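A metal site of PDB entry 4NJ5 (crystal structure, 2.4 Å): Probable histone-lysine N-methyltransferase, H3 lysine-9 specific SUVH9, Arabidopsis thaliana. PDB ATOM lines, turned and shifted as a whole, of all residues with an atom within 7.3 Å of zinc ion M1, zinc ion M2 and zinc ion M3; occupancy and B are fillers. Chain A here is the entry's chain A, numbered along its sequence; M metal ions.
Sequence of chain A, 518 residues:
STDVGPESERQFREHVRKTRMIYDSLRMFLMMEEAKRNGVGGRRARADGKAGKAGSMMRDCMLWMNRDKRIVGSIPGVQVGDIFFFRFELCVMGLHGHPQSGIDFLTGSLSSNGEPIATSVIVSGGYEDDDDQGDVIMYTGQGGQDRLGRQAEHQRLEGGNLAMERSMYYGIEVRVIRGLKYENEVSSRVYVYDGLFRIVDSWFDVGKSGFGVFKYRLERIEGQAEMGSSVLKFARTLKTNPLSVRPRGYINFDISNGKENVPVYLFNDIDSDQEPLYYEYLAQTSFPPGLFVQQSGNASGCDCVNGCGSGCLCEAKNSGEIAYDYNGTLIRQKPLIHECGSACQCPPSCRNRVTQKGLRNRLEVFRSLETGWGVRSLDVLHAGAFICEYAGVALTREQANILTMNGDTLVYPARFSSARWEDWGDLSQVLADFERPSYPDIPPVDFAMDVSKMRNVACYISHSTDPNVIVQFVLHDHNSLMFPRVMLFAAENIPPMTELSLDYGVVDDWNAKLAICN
The guanidinium group (NE) of Arg 351 is in hydrogen-bond range of the backbone carbonyl oxygen (O) of Cys 308.
SG of Cys 312 lies close to N of Cys 314 (3.4 Å).
O of Cys 302 lies within hydrogen-bond range of N of Gln 345, 2.9 Å away.
The guanidinium group (NH2) of Arg 353 sits at hydrogen-bond distance from the backbone carbonyl oxygen (O) of Cys 346.
O of Asn 352 lies within hydrogen-bond range of N of Cys 340 (3.0 Å).
The backbone carbonyl oxygen of Cys 340 sits at hydrogen-bond distance from the guanidinium group of Arg 353, 3.3 Å away.
SG of Cys 350 sits close to N of Asn 352 (3.2 Å).
The side-chain sulfur (SG) of Cys 312 lies close to the backbone NH (N) of Glu 315 (3.6 Å).
Of the 31 residues printed, 5 come within 4 Å of zinc ion M1.
The nearest printed residue that does not touch zinc ion M2 is Cys 346 (4.2 Å).
Zinc ion M1 is bound by SG of Cys 308 (2.3 Å), SG of Cys 346 (2.3 Å), SG of Cys 350 (2.4 Å) and SG of Cys 340 (2.4 Å).
Zinc ion M1 has four donor atoms within binding distance.
Zinc ion M2 is bound by SG of Cys 314 (2.3 Å), SG of Cys 302 (2.3 Å), SG of Cys 340 (2.4 Å) and SG of Cys 344 (2.4 Å).
Zinc ion M2 has four donor atoms within binding distance.
Zinc ion M3 is bound by SG of Cys 308 (2.3 Å), SG of Cys 304 (2.3 Å), SG of Cys 312 (2.4 Å) and SG of Cys 302 (2.6 Å).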
ATOM      1  N   SER A 300      23.175   3.392  24.771  1.00  0.00           N
ATOM      2  CA  SER A 300      23.937   4.258  23.888  1.00  0.00           C
ATOM      3  C   SER A 300      23.453   4.141  22.442  1.00  0.00           C
ATOM      4  O   SER A 300      23.019   3.068  22.015  1.00  0.00           O
ATOM      5  CB  SER A 300      25.398   3.884  23.985  1.00  0.00           C
ATOM      6  OG  SER A 300      25.509   2.482  23.981  1.00  0.00           O
ATOM      7  N   GLY A 301      23.525   5.244  21.705  1.00  0.00           N
ATOM      8  CA  GLY A 301      23.100   5.276  20.314  1.00  0.00           C
ATOM      9  C   GLY A 301      24.274   5.535  19.393  1.00  0.00           C
ATOM     10  O   GLY A 301      25.349   5.948  19.836  1.00  0.00           O
ATOM     11  N   CYS A 302      24.079   5.281  18.100  1.00  0.00           N
ATOM     12  CA  CYS A 302      25.109   5.587  17.125  1.00  0.00           C
ATOM     13  C   CYS A 302      25.116   7.085  16.811  1.00  0.00           C
ATOM     14  O   CYS A 302      24.199   7.822  17.202  1.00  0.00           O
ATOM     15  CB  CYS A 302      24.940   4.769  15.847  1.00  0.00           C
ATOM     16  SG  CYS A 302      23.457   5.165  14.923  1.00  0.00           S
ATOM     17  N   ASP A 303      26.151   7.529  16.112  1.00  0.00           N
ATOM     18  CA  ASP A 303      26.339   8.950  15.813  1.00  0.00           C
ATOM     19  C   ASP A 303      26.280   9.241  14.322  1.00  0.00           C
ATOM     20  O   ASP A 303      27.001  10.106  13.818  1.00  0.00           O
ATOM     21  CB  ASP A 303      27.688   9.422  16.382  1.00  0.00           C
ATOM     22  CG  ASP A 303      28.865   8.628  15.846  1.00  0.00           C
ATOM     23  OD1 ASP A 303      28.637   7.658  15.091  1.00  0.00           O
ATOM     24  OD2 ASP A 303      30.014   8.963  16.193  1.00  0.00           O
ATOM     25  N   CYS A 304      25.415   8.516  13.611  1.00  0.00           N
ATOM     26  CA  CYS A 304      25.316   8.619  12.161  1.00  0.00           C
ATOM     27  C   CYS A 304      24.394   9.741  11.710  1.00  0.00           C
ATOM     28  O   CYS A 304      23.305   9.485  11.204  1.00  0.00           O
ATOM     29  CB  CYS A 304      24.844   7.289  11.562  1.00  0.00           C
ATOM     30  SG  CYS A 304      25.934   5.911  11.941  1.00  0.00           S
ATOM     31  N   VAL A 305      24.850  10.974  11.871  1.00  0.00           N
ATOM     32  CA  VAL A 305      24.031  12.156  11.627  1.00  0.00           C
ATOM     33  C   VAL A 305      23.485  12.278  10.203  1.00  0.00           C
ATOM     34  O   VAL A 305      22.593  13.082   9.941  1.00  0.00           O
ATOM     35  CB  VAL A 305      24.788  13.437  12.001  1.00  0.00           C
ATOM     36  CG1 VAL A 305      25.180  13.398  13.470  1.00  0.00           C
ATOM     37  CG2 VAL A 305      26.015  13.601  11.122  1.00  0.00           C
ATOM     38  N   GLY A 307      22.490   9.297   8.600  1.00  0.00           N
ATOM     39  CA  GLY A 307      21.905   7.991   8.392  1.00  0.00           C
ATOM     40  C   GLY A 307      22.931   6.883   8.551  1.00  0.00           C
ATOM     41  O   GLY A 307      24.102   7.075   8.206  1.00  0.00           O
ATOM     42  N   CYS A 308      22.507   5.741   9.075  1.00  0.00           N
ATOM     43  CA  CYS A 308      23.427   4.623   9.268  1.00  0.00           C
ATOM     44  C   CYS A 308      23.959   4.109   7.941  1.00  0.00           C
ATOM     45  O   CYS A 308      23.195   3.811   7.030  1.00  0.00           O
ATOM     46  CB  CYS A 308      22.764   3.475  10.040  1.00  0.00           C
ATOM     47  SG  CYS A 308      22.537   3.792  11.800  1.00  0.00           S
ATOM     48  N   GLY A 309      25.278   4.021   7.848  1.00  0.00           N
ATOM     49  CA  GLY A 309      25.930   3.408   6.702  1.00  0.00           C
ATOM     50  C   GLY A 309      26.611   2.125   7.139  1.00  0.00           C
ATOM     51  O   GLY A 309      25.939   1.130   7.406  1.00  0.00           O
ATOM     52  N   SER A 310      27.932   2.158   7.245  1.00  0.00           N
ATOM     53  CA  SER A 310      28.711   0.988   7.642  1.00  0.00           C
ATOM     54  C   SER A 310      29.688   1.320   8.767  1.00  0.00           C
ATOM     55  O   SER A 310      30.241   2.416   8.817  1.00  0.00           O
ATOM     56  CB  SER A 310      29.491   0.426   6.458  1.00  0.00           C
ATOM     57  OG  SER A 310      28.636  -0.281   5.566  1.00  0.00           O
ATOM     58  N   GLY A 311      29.908   0.361   9.666  1.00  0.00           N
ATOM     59  CA  GLY A 311      30.924   0.492  10.685  1.00  0.00           C
ATOM     60  C   GLY A 311      30.552   1.285  11.911  1.00  0.00           C
ATOM     61  O   GLY A 311      31.421   1.696  12.679  1.00  0.00           O
ATOM     62  N   CYS A 312      29.253   1.519  12.121  1.00  0.00           N
ATOM     63  CA  CYS A 312      28.817   2.225  13.319  1.00  0.00           C
ATOM     64  C   CYS A 312      28.483   1.250  14.452  1.00  0.00           C
ATOM     65  O   CYS A 312      28.491   0.030  14.266  1.00  0.00           O
ATOM     66  CB  CYS A 312      27.630   3.136  13.019  1.00  0.00           C
ATOM     67  SG  CYS A 312      26.003   2.356  13.151  1.00  0.00           S
ATOM     68  N   LEU A 313      28.202   1.811  15.628  1.00  0.00           N
ATOM     69  CA  LEU A 313      27.911   1.022  16.823  1.00  0.00           C
ATOM     70  C   LEU A 313      26.682   0.128  16.653  1.00  0.00           C
ATOM     71  O   LEU A 313      26.703  -1.044  17.033  1.00  0.00           O
ATOM     72  CB  LEU A 313      27.713   1.963  18.027  1.00  0.00           C
ATOM     73  CG  LEU A 313      26.732   1.543  19.123  1.00  0.00           C
ATOM     74  CD1 LEU A 313      27.291   0.421  19.971  1.00  0.00           C
ATOM     75  CD2 LEU A 313      26.334   2.739  19.976  1.00  0.00           C
ATOM     76  N   CYS A 314      25.623   0.690  16.080  1.00  0.00           N
ATOM     77  CA  CYS A 314      24.392  -0.060  15.873  1.00  0.00           C
ATOM     78  C   CYS A 314      24.577  -1.241  14.921  1.00  0.00           C
ATOM     79  O   CYS A 314      23.896  -2.258  15.049  1.00  0.00           O
ATOM     80  CB  CYS A 314      23.276   0.865  15.402  1.00  0.00           C
ATOM     81  SG  CYS A 314      22.682   1.966  16.706  1.00  0.00           S
ATOM     82  N   GLU A 315      25.515  -1.122  13.982  1.00  0.00           N
ATOM     83  CA  GLU A 315      25.858  -2.259  13.141  1.00  0.00           C
ATOM     84  C   GLU A 315      26.525  -3.353  13.964  1.00  0.00           C
ATOM     85  O   GLU A 315      26.251  -4.536  13.796  1.00  0.00           O
ATOM     86  CB  GLU A 315      26.752  -1.843  11.974  1.00  0.00           C
ATOM     87  CG  GLU A 315      27.206  -3.020  11.125  1.00  0.00           C
ATOM     88  CD  GLU A 315      27.824  -2.606   9.803  1.00  0.00           C
ATOM     89  OE1 GLU A 315      27.108  -2.606   8.790  1.00  0.00           O
ATOM     90  OE2 GLU A 315      29.040  -2.282   9.782  1.00  0.00           O
ATOM     91  N   LYS A 317      25.991  -3.873  17.057  1.00  0.00           N
ATOM     92  CA  LYS A 317      24.911  -4.448  17.855  1.00  0.00           C
ATOM     93  C   LYS A 317      24.165  -5.521  17.061  1.00  0.00           C
ATOM     94  O   LYS A 317      23.603  -6.451  17.634  1.00  0.00           O
ATOM     95  CB  LYS A 317      23.935  -3.367  18.339  1.00  0.00           C
ATOM     96  CG  LYS A 317      24.574  -2.271  19.193  1.00  0.00           C
ATOM     97  CD  LYS A 317      23.554  -1.182  19.576  1.00  0.00           C
ATOM     98  CE  LYS A 317      22.571  -1.674  20.626  1.00  0.00           C
ATOM     99  NZ  LYS A 317      21.295  -0.903  20.618  1.00  0.00           N
ATOM    100  N   ILE A 322      23.664  -4.362   9.444  1.00  0.00           N
ATOM    101  CA  ILE A 322      22.387  -3.670   9.575  1.00  0.00           C
ATOM    102  C   ILE A 322      21.302  -4.494   8.893  1.00  0.00           C
ATOM    103  O   ILE A 322      21.446  -4.906   7.750  1.00  0.00           O
ATOM    104  CB  ILE A 322      22.443  -2.267   8.932  1.00  0.00           C
ATOM    105  CG1 ILE A 322      23.527  -1.419   9.595  1.00  0.00           C
ATOM    106  CG2 ILE A 322      21.093  -1.577   9.056  1.00  0.00           C
ATOM    107  CD1 ILE A 322      23.157  -0.943  10.995  1.00  0.00           C
ATOM    108  N   HIS A 338      18.263  -4.905  16.221  1.00  0.00           N
ATOM    109  CA  HIS A 338      18.408  -3.661  16.981  1.00  0.00           C
ATOM    110  C   HIS A 338      18.269  -2.458  16.051  1.00  0.00           C
ATOM    111  O   HIS A 338      19.207  -2.110  15.327  1.00  0.00           O
ATOM    112  CB  HIS A 338      19.767  -3.613  17.693  1.00  0.00           C
ATOM    113  CG  HIS A 338      19.986  -4.715  18.679  1.00  0.00           C
ATOM    114  ND1 HIS A 338      19.664  -4.593  20.020  1.00  0.00           N
ATOM    115  CD2 HIS A 338      20.498  -5.959  18.529  1.00  0.00           C
ATOM    116  CE1 HIS A 338      19.968  -5.712  20.645  1.00  0.00           C
ATOM    117  NE2 HIS A 338      20.476  -6.560  19.772  1.00  0.00           N
ATOM    118  N   GLU A 339      17.105  -1.838  16.060  1.00  0.00           N
ATOM    119  CA  GLU A 339      16.894  -0.612  15.296  1.00  0.00           C
ATOM    120  C   GLU A 339      17.431   0.569  16.084  1.00  0.00           C
ATOM    121  O   GLU A 339      17.612   0.490  17.293  1.00  0.00           O
ATOM    122  CB  GLU A 339      15.406  -0.409  14.972  1.00  0.00           C
ATOM    123  CG  GLU A 339      14.908  -1.298  13.841  1.00  0.00           C
ATOM    124  CD  GLU A 339      13.475  -0.997  13.433  1.00  0.00           C
ATOM    125  OE1 GLU A 339      12.923   0.034  13.875  1.00  0.00           O
ATOM    126  OE2 GLU A 339      12.917  -1.806  12.656  1.00  0.00           O
ATOM    127  N   CYS A 340      17.694   1.677  15.389  1.00  0.00           N
ATOM    128  CA  CYS A 340      18.123   2.894  16.060  1.00  0.00           C
ATOM    129  C   CYS A 340      16.980   3.471  16.886  1.00  0.00           C
ATOM    130  O   CYS A 340      15.812   3.354  16.505  1.00  0.00           O
ATOM    131  CB  CYS A 340      18.606   3.921  15.043  1.00  0.00           C
ATOM    132  SG  CYS A 340      20.020   3.362  14.092  1.00  0.00           S
ATOM    133  N   GLY A 341      17.323   4.066  18.014  1.00  0.00           N
ATOM    134  CA  GLY A 341      16.324   4.678  18.879  1.00  0.00           C
ATOM    135  C   GLY A 341      16.638   6.131  19.185  1.00  0.00           C
ATOM    136  O   GLY A 341      17.414   6.773  18.467  1.00  0.00           O
ATOM    137  N   ALA A 343      18.393   7.413  21.434  1.00  0.00           N
ATOM    138  CA  ALA A 343      19.796   7.636  21.770  1.00  0.00           C
ATOM    139  C   ALA A 343      20.661   7.802  20.517  1.00  0.00           C
ATOM    140  O   ALA A 343      21.761   8.342  20.581  1.00  0.00           O
ATOM    141  CB  ALA A 343      20.325   6.507  22.646  1.00  0.00           C
ATOM    142  N   CYS A 344      20.153   7.353  19.370  1.00  0.00           N
ATOM    143  CA  CYS A 344      20.879   7.513  18.120  1.00  0.00           C
ATOM    144  C   CYS A 344      20.699   8.898  17.515  1.00  0.00           C
ATOM    145  O   CYS A 344      19.653   9.538  17.688  1.00  0.00           O
ATOM    146  CB  CYS A 344      20.474   6.430  17.115  1.00  0.00           C
ATOM    147  SG  CYS A 344      20.825   4.754  17.687  1.00  0.00           S
ATOM    148  N   GLN A 345      21.721   9.367  16.808  1.00  0.00           N
ATOM    149  CA  GLN A 345      21.729  10.719  16.263  1.00  0.00           C
ATOM    150  C   GLN A 345      21.377  10.731  14.781  1.00  0.00           C
ATOM    151  O   GLN A 345      21.401  11.782  14.143  1.00  0.00           O
ATOM    152  CB  GLN A 345      23.079  11.384  16.511  1.00  0.00           C
ATOM    153  CG  GLN A 345      23.354  11.642  17.977  1.00  0.00           C
ATOM    154  CD  GLN A 345      24.787  12.059  18.238  1.00  0.00           C
ATOM    155  OE1 GLN A 345      25.717  11.272  18.068  1.00  0.00           O
ATOM    156  NE2 GLN A 345      24.981  13.296  18.663  1.00  0.00           N
ATOM    157  N   CYS A 346      21.051   9.564  14.235  1.00  0.00           N
ATOM    158  CA  CYS A 346      20.576   9.485  12.863  1.00  0.00           C
ATOM    159  C   CYS A 346      19.161  10.045  12.777  1.00  0.00           C
ATOM    160  O   CYS A 346      18.402   9.963  13.744  1.00  0.00           O
ATOM    161  CB  CYS A 346      20.640   8.047  12.345  1.00  0.00           C
ATOM    162  SG  CYS A 346      19.897   6.821  13.426  1.00  0.00           S
ATOM    163  N   PRO A 347      18.807  10.630  11.621  1.00  0.00           N
ATOM    164  CA  PRO A 347      17.467  11.181  11.371  1.00  0.00           C
ATOM    165  C   PRO A 347      16.455  10.067  11.131  1.00  0.00           C
ATOM    166  O   PRO A 347      16.841   8.901  11.034  1.00  0.00           O
ATOM    167  CB  PRO A 347      17.681  11.989  10.089  1.00  0.00           C
ATOM    168  CG  PRO A 347      18.797  11.296   9.391  1.00  0.00           C
ATOM    169  CD  PRO A 347      19.716  10.851  10.484  1.00  0.00           C
ATOM    170  N   SER A 349      15.016   9.266   8.522  1.00  0.00           N
ATOM    171  CA  SER A 349      15.211   8.631   7.216  1.00  0.00           C
ATOM    172  C   SER A 349      16.254   7.513   7.230  1.00  0.00           C
ATOM    173  O   SER A 349      16.456   6.846   6.218  1.00  0.00           O
ATOM    174  CB  SER A 349      15.611   9.683   6.170  1.00  0.00           C
ATOM    175  OG  SER A 349      16.942  10.104   6.380  1.00  0.00           O
ATOM    176  N   CYS A 350      16.918   7.322   8.363  1.00  0.00           N
ATOM    177  CA  CYS A 350      17.922   6.266   8.490  1.00  0.00           C
ATOM    178  C   CYS A 350      17.356   4.882   8.154  1.00  0.00           C
ATOM    179  O   CYS A 350      16.242   4.540   8.559  1.00  0.00           O
ATOM    180  CB  CYS A 350      18.518   6.248   9.888  1.00  0.00           C
ATOM    181  SG  CYS A 350      19.534   4.790  10.206  1.00  0.00           S
ATOM    182  N   ARG A 351      18.129   4.089   7.432  1.00  0.00           N
ATOM    183  CA  ARG A 351      17.684   2.757   7.004  1.00  0.00           C
ATOM    184  C   ARG A 351      17.490   1.784   8.164  1.00  0.00           C
ATOM    185  O   ARG A 351      16.911   0.716   7.998  1.00  0.00           O
ATOM    186  CB  ARG A 351      18.663   2.158   5.986  1.00  0.00           C
ATOM    187  CG  ARG A 351      19.993   1.714   6.586  1.00  0.00           C
ATOM    188  CD  ARG A 351      20.870   1.041   5.537  1.00  0.00           C
ATOM    189  NE  ARG A 351      22.242   0.873   6.000  1.00  0.00           N
ATOM    190  CZ  ARG A 351      22.880  -0.289   6.030  1.00  0.00           C
ATOM    191  NH1 ARG A 351      22.284  -1.396   5.626  1.00  0.00           N
ATOM    192  NH2 ARG A 351      24.137  -0.346   6.456  1.00  0.00           N
ATOM    193  N   ASN A 352      17.979   2.136   9.347  1.00  0.00           N
ATOM    194  CA  ASN A 352      17.838   1.256  10.502  1.00  0.00           C
ATOM    195  C   ASN A 352      16.671   1.659  11.399  1.00  0.00           C
ATOM    196  O   ASN A 352      16.705   1.450  12.618  1.00  0.00           O
ATOM    197  CB  ASN A 352      19.147   1.177  11.297  1.00  0.00           C
ATOM    198  CG  ASN A 352      19.224  -0.070  12.152  1.00  0.00           C
ATOM    199  OD1 ASN A 352      18.649  -1.103  11.806  1.00  0.00           O
ATOM    200  ND2 ASN A 352      19.931   0.024  13.269  1.00  0.00           N
ATOM    201  N   ARG A 353      15.635   2.243  10.798  1.00  0.00           N
ATOM    202  CA  ARG A 353      14.438   2.640  11.530  1.00  0.00           C
ATOM    203  C   ARG A 353      13.168   2.169  10.829  1.00  0.00           C
ATOM    204  O   ARG A 353      12.210   2.922  10.691  1.00  0.00           O
ATOM    205  CB  ARG A 353      14.401   4.170  11.710  1.00  0.00           C
ATOM    206  CG  ARG A 353      15.498   4.751  12.586  1.00  0.00           C
ATOM    207  CD  ARG A 353      15.309   6.245  12.790  1.00  0.00           C
ATOM    208  NE  ARG A 353      16.374   6.867  13.580  1.00  0.00           N
ATOM    209  CZ  ARG A 353      16.362   6.976  14.900  1.00  0.00           C
ATOM    210  NH1 ARG A 353      15.349   6.485  15.600  1.00  0.00           N
ATOM    211  NH2 ARG A 353      17.368   7.560  15.534  1.00  0.00           N
HETATM  212 ZN    ZN M   1      20.590   4.883  12.323  1.00  0.00          ZN
HETATM  213 ZN    ZN M   2      21.740   3.778  15.654  1.00  0.00          ZN
HETATM  214 ZN    ZN M   3      24.556   4.276  12.790  1.00  0.00          ZN
